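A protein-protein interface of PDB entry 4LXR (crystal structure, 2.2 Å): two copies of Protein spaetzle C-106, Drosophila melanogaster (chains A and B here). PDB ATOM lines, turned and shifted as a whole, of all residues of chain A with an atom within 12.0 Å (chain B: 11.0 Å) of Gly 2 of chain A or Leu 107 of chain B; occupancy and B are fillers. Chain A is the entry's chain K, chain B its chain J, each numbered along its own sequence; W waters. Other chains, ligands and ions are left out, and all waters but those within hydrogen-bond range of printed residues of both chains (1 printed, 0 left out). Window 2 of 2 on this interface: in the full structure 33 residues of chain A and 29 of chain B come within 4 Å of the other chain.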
ATOM      1  N   VAL A   1      15.850  -9.617   3.342  1.00  0.00           N
ATOM      2  CA  VAL A   1      15.039  -8.532   3.885  1.00  0.00           C
ATOM      3  C   VAL A   1      15.780  -7.201   3.728  1.00  0.00           C
ATOM      4  O   VAL A   1      16.771  -7.116   2.986  1.00  0.00           O
ATOM      5  CB  VAL A   1      14.725  -8.778   5.372  1.00  0.00           C
ATOM      6  CG1 VAL A   1      13.314  -8.290   5.718  1.00  0.00           C
ATOM      7  CG2 VAL A   1      14.881 -10.261   5.703  1.00  0.00           C
ATOM      8  N   GLY A   2      15.309  -6.167   4.421  1.00  0.00           N
ATOM      9  CA  GLY A   2      15.995  -4.885   4.413  1.00  0.00           C
ATOM     10  C   GLY A   2      17.322  -4.877   5.162  1.00  0.00           C
ATOM     11  O   GLY A   2      17.528  -5.661   6.089  1.00  0.00           O
ATOM     12  N   GLY A   3      18.228  -3.991   4.752  1.00  0.00           N
ATOM     13  CA  GLY A   3      19.493  -3.796   5.445  1.00  0.00           C
ATOM     14  C   GLY A   3      20.678  -4.602   4.931  1.00  0.00           C
ATOM     15  O   GLY A   3      21.775  -4.522   5.479  1.00  0.00           O
ATOM     16  N   SER A   4      20.472  -5.395   3.889  1.00  0.00           N
ATOM     17  CA  SER A   4      21.575  -6.172   3.323  1.00  0.00           C
ATOM     18  C   SER A   4      22.299  -5.377   2.238  1.00  0.00           C
ATOM     19  O   SER A   4      21.768  -4.406   1.700  1.00  0.00           O
ATOM     20  CB  SER A   4      21.080  -7.508   2.763  1.00  0.00           C
ATOM     21  OG  SER A   4      20.309  -7.302   1.593  1.00  0.00           O
ATOM     22  N   ASP A   5      23.511  -5.800   1.915  1.00  0.00           N
ATOM     23  CA  ASP A   5      24.333  -5.082   0.961  1.00  0.00           C
ATOM     24  C   ASP A   5      25.447  -6.017   0.532  1.00  0.00           C
ATOM     25  O   ASP A   5      26.096  -6.635   1.364  1.00  0.00           O
ATOM     26  CB  ASP A   5      24.929  -3.851   1.636  1.00  0.00           C
ATOM     27  CG  ASP A   5      25.660  -2.936   0.670  1.00  0.00           C
ATOM     28  OD1 ASP A   5      25.231  -2.785  -0.499  1.00  0.00           O
ATOM     29  OD2 ASP A   5      26.659  -2.344   1.102  1.00  0.00           O
ATOM     30  N   GLU A   6      25.670  -6.128  -0.766  1.00  0.00           N
ATOM     31  CA  GLU A   6      26.756  -6.957  -1.271  1.00  0.00           C
ATOM     32  C   GLU A   6      27.991  -6.099  -1.438  1.00  0.00           C
ATOM     33  O   GLU A   6      27.922  -4.995  -1.954  1.00  0.00           O
ATOM     34  CB  GLU A   6      26.380  -7.559  -2.620  1.00  0.00           C
ATOM     35  CG  GLU A   6      25.224  -8.505  -2.564  1.00  0.00           C
ATOM     36  CD  GLU A   6      25.014  -9.211  -3.891  1.00  0.00           C
ATOM     37  OE1 GLU A   6      25.383  -8.626  -4.932  1.00  0.00           O
ATOM     38  OE2 GLU A   6      24.498 -10.349  -3.888  1.00  0.00           O
ATOM     39  N   ARG A   7      29.125  -6.597  -0.985  1.00  0.00           N
ATOM     40  CA  ARG A   7      30.357  -5.864  -1.163  1.00  0.00           C
ATOM     41  C   ARG A   7      31.216  -6.626  -2.171  1.00  0.00           C
ATOM     42  O   ARG A   7      31.188  -7.847  -2.220  1.00  0.00           O
ATOM     43  CB  ARG A   7      31.093  -5.729   0.168  1.00  0.00           C
ATOM     44  CG  ARG A   7      30.273  -5.080   1.267  1.00  0.00           C
ATOM     45  CD  ARG A   7      29.852  -3.639   0.924  1.00  0.00           C
ATOM     46  NE  ARG A   7      30.972  -2.700   0.916  1.00  0.00           N
ATOM     47  CZ  ARG A   7      31.486  -2.141   2.019  1.00  0.00           C
ATOM     48  NH1 ARG A   7      32.497  -1.291   1.929  1.00  0.00           N
ATOM     49  NH2 ARG A   7      30.998  -2.453   3.216  1.00  0.00           N
ATOM     50  N   SER B  63      31.638 -11.697   9.463  1.00  0.00           N
ATOM     51  CA  SER B  63      30.324 -11.165   9.084  1.00  0.00           C
ATOM     52  C   SER B  63      30.087 -11.117   7.580  1.00  0.00           C
ATOM     53  O   SER B  63      28.969 -10.870   7.135  1.00  0.00           O
ATOM     54  CB  SER B  63      30.052  -9.793   9.704  1.00  0.00           C
ATOM     55  OG  SER B  63      30.681  -8.750   8.975  1.00  0.00           O
ATOM     56  N   TYR B  64      31.137 -11.335   6.799  1.00  0.00           N
ATOM     57  CA  TYR B  64      30.999 -11.366   5.339  1.00  0.00           C
ATOM     58  C   TYR B  64      30.801 -12.807   4.857  1.00  0.00           C
ATOM     59  O   TYR B  64      31.556 -13.698   5.218  1.00  0.00           O
ATOM     60  CB  TYR B  64      32.206 -10.719   4.651  1.00  0.00           C
ATOM     61  CG  TYR B  64      32.379  -9.257   5.012  1.00  0.00           C
ATOM     62  CD1 TYR B  64      31.707  -8.271   4.316  1.00  0.00           C
ATOM     63  CD2 TYR B  64      33.205  -8.870   6.069  1.00  0.00           C
ATOM     64  CE1 TYR B  64      31.851  -6.910   4.652  1.00  0.00           C
ATOM     65  CE2 TYR B  64      33.359  -7.527   6.424  1.00  0.00           C
ATOM     66  CZ  TYR B  64      32.681  -6.555   5.712  1.00  0.00           C
ATOM     67  OH  TYR B  64      32.831  -5.227   6.051  1.00  0.00           O
ATOM     68  N   ASN B  65      29.758 -13.019   4.071  1.00  0.00           N
ATOM     69  CA  ASN B  65      29.444 -14.319   3.517  1.00  0.00           C
ATOM     70  C   ASN B  65      29.748 -14.281   2.021  1.00  0.00           C
ATOM     71  O   ASN B  65      29.003 -13.673   1.268  1.00  0.00           O
ATOM     72  CB  ASN B  65      27.969 -14.639   3.759  1.00  0.00           C
ATOM     73  CG  ASN B  65      27.533 -15.952   3.108  1.00  0.00           C
ATOM     74  OD1 ASN B  65      28.283 -16.931   3.086  1.00  0.00           O
ATOM     75  ND2 ASN B  65      26.317 -15.972   2.571  1.00  0.00           N
ATOM     76  N   LEU B 103      30.541 -10.274  -1.304  1.00  0.00           N
ATOM     77  CA  LEU B 103      30.592 -10.469   0.138  1.00  0.00           C
ATOM     78  C   LEU B 103      29.266  -9.983   0.681  1.00  0.00           C
ATOM     79  O   LEU B 103      29.042  -8.781   0.785  1.00  0.00           O
ATOM     80  CB  LEU B 103      31.764  -9.699   0.780  1.00  0.00           C
ATOM     81  CG  LEU B 103      33.181  -9.991   0.252  1.00  0.00           C
ATOM     82  CD1 LEU B 103      34.272  -9.362   1.128  1.00  0.00           C
ATOM     83  CD2 LEU B 103      33.447 -11.481   0.110  1.00  0.00           C
ATOM     84  N   LYS B 104      28.366 -10.909   0.978  1.00  0.00           N
ATOM     85  CA  LYS B 104      27.066 -10.521   1.493  1.00  0.00           C
ATOM     86  C   LYS B 104      27.179 -10.117   2.960  1.00  0.00           C
ATOM     87  O   LYS B 104      27.873 -10.788   3.743  1.00  0.00           O
ATOM     88  CB  LYS B 104      26.074 -11.667   1.352  1.00  0.00           C
ATOM     89  CG  LYS B 104      25.799 -12.051  -0.098  1.00  0.00           C
ATOM     90  CD  LYS B 104      24.974 -13.311  -0.172  1.00  0.00           C
ATOM     91  CE  LYS B 104      23.953 -13.233  -1.297  1.00  0.00           C
ATOM     92  NZ  LYS B 104      24.577 -12.883  -2.603  1.00  0.00           N
ATOM     93  N   THR B 105      26.512  -9.030   3.310  1.00  0.00           N
ATOM     94  CA  THR B 105      26.339  -8.636   4.696  1.00  0.00           C
ATOM     95  C   THR B 105      24.864  -8.389   4.947  1.00  0.00           C
ATOM     96  O   THR B 105      24.092  -8.165   4.010  1.00  0.00           O
ATOM     97  CB  THR B 105      27.091  -7.335   5.017  1.00  0.00           C
ATOM     98  OG1 THR B 105      26.704  -6.310   4.089  1.00  0.00           O
ATOM     99  CG2 THR B 105      28.555  -7.558   4.905  1.00  0.00           C
ATOM    100  N   GLY B 106      24.476  -8.421   6.213  1.00  0.00           N
ATOM    101  CA  GLY B 106      23.116  -8.088   6.585  1.00  0.00           C
ATOM    102  C   GLY B 106      23.025  -7.614   8.023  1.00  0.00           C
ATOM    103  O   GLY B 106      24.024  -7.571   8.733  1.00  0.00           O
ATOM    104  N   LEU B 107      21.816  -7.265   8.446  1.00  0.00           N
ATOM    105  CA  LEU B 107      21.577  -6.815   9.815  1.00  0.00           C
ATOM    106  C   LEU B 107      21.660  -7.982  10.810  1.00  0.00           C
ATOM    107  O   LEU B 107      22.291  -7.871  11.866  1.00  0.00           O
ATOM    108  CB  LEU B 107      20.225  -6.097   9.912  1.00  0.00           C
ATOM    109  CG  LEU B 107      20.185  -4.591   9.610  1.00  0.00           C
ATOM    110  CD1 LEU B 107      21.308  -4.149   8.668  1.00  0.00           C
ATOM    111  CD2 LEU B 107      18.816  -4.182   9.057  1.00  0.00           C
ATOM    112  N   GLU B 108      21.042  -9.106  10.456  1.00  0.00           N
ATOM    113  CA  GLU B 108      21.090 -10.301  11.293  1.00  0.00           C
ATOM    114  C   GLU B 108      22.500 -10.878  11.371  1.00  0.00           C
ATOM    115  O   GLU B 108      23.221 -10.936  10.370  1.00  0.00           O
ATOM    116  CB  GLU B 108      20.097 -11.352  10.794  1.00  0.00           C
ATOM    117  CG  GLU B 108      18.643 -10.962  11.013  1.00  0.00           C
ATOM    118  CD  GLU B 108      17.666 -11.998  10.484  1.00  0.00           C
ATOM    119  OE1 GLU B 108      17.833 -13.202  10.798  1.00  0.00           O
ATOM    120  OE2 GLU B 108      16.733 -11.605   9.751  1.00  0.00           O
ATOM    121  N   HIS B 109      22.886 -11.312  12.564  1.00  0.00           N
ATOM    122  CA  HIS B 109      24.268 -11.711  12.817  1.00  0.00           C
ATOM    123  C   HIS B 109      24.755 -12.984  12.089  1.00  0.00           C
ATOM    124  O   HIS B 109      25.677 -12.927  11.269  1.00  0.00           O
ATOM    125  CB  HIS B 109      24.528 -11.808  14.321  1.00  0.00           C
ATOM    126  CG  HIS B 109      25.963 -12.041  14.664  1.00  0.00           C
ATOM    127  ND1 HIS B 109      26.481 -13.303  14.871  1.00  0.00           N
ATOM    128  CD2 HIS B 109      26.997 -11.180  14.819  1.00  0.00           C
ATOM    129  CE1 HIS B 109      27.767 -13.207  15.147  1.00  0.00           C
ATOM    130  NE2 HIS B 109      28.107 -11.930  15.124  1.00  0.00           N
ATOM    131  N   HIS B 110      24.149 -14.127  12.386  1.00  0.00           N
ATOM    132  CA  HIS B 110      24.631 -15.379  11.811  1.00  0.00           C
ATOM    133  C   HIS B 110      23.500 -16.379  11.578  1.00  0.00           C
ATOM    134  O   HIS B 110      23.268 -16.818  10.449  1.00  0.00           O
ATOM    135  CB  HIS B 110      25.711 -15.988  12.712  1.00  0.00           C
ATOM    136  CG  HIS B 110      26.688 -16.862  11.986  1.00  0.00           C
ATOM    137  ND1 HIS B 110      28.050 -16.780  12.188  1.00  0.00           N
ATOM    138  CD2 HIS B 110      26.502 -17.840  11.067  1.00  0.00           C
ATOM    139  CE1 HIS B 110      28.660 -17.666  11.420  1.00  0.00           C
ATOM    140  NE2 HIS B 110      27.744 -18.322  10.731  1.00  0.00           N
HETATM  141  O   HOH W   1      19.697  -7.346   6.328  1.00  0.00           O
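N of Leu 103 of chain B lies within hydrogen-bond range of O of Arg 7 of chain A (2.7 Å). The side-chain carboxylate (OE2) of Glu 6 of chain A is in salt-bridge range of the side-chain amino group (NZ) of Lys 104 of chain B (2.8 Å). The side-chain hydroxyl of Thr 105 of chain B lies within hydrogen-bond range of the backbone carbonyl oxygen of Asp 5 of chain A (2.8 Å).
The backbone carbonyl oxygen (O) of Asn 65 of chain B sits at hydrogen-bond distance from the backbone NH (N) of Lys 104 of chain B (2.9 Å).
Leu 107 of chain B touches Gly 2 of chain A. Gly 3 of chain A touches Gly 106 of chain B (O to CA, 3.97 Å). Gly 3 of chain A touches Leu 107 of chain B (O to CD1, 3.2 Å). Thr 105 of chain B touches Ser 4 of chain A. Leu 103 of chain B touches Asp 5 of chain A. O of Asp 5 of chain A touches C of Lys 104 of chain B (3.98 Å). Glu 6 of chain A touches Leu 103 of chain B (CA to O, 3.6 Å).
No residue of chain B comes within 4 Å of Val 1 of chain A. Gly 2 of chain A touches one residue of chain B. Gly 3 of chain A touches just these residues of chain B: Gly 106 and Leu 107. Of the printed residues of chain B, Arg 7 of chain A touches Leu 103 (2.7 Å). Of the printed residues of chain A, Lys 104 of chain B touches Asp 5 and Glu 6. Thr 105 of chain B touches two residues of chain A. Gly 106 of chain B touches just one residue of chain A: Gly 3 (3.97 Å). Of chain A, only Gly 2 and Gly 3 come within 4 Å of Leu 107 of chain B. The nearest residue of chain B that does not touch Gly 2 of chain A is Gly 106 of chain B (6.1 Å). The nearest residue of chain A that does not touch Leu 107 of chain B is Ser 4 of chain A (5.0 Å).
Of the 7 printed residues of chain A, 6 touch a printed residue of chain B. Hydrophobic or aromatic side chains of chain B that line the printed part of chain A: Leu 103 and Leu 107.
No position is printed for both chains. Of the 10 pairs that touch across the chains among the printed residues, none has its exchanged pair printed and touching as well.
Water W1 lies within hydrogen-bond range of O of Gly 2 of chain A (2.8 Å), N of Leu 107 of chain B (3.0 Å) and N of Ser 4 of chain A (3.2 Å).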
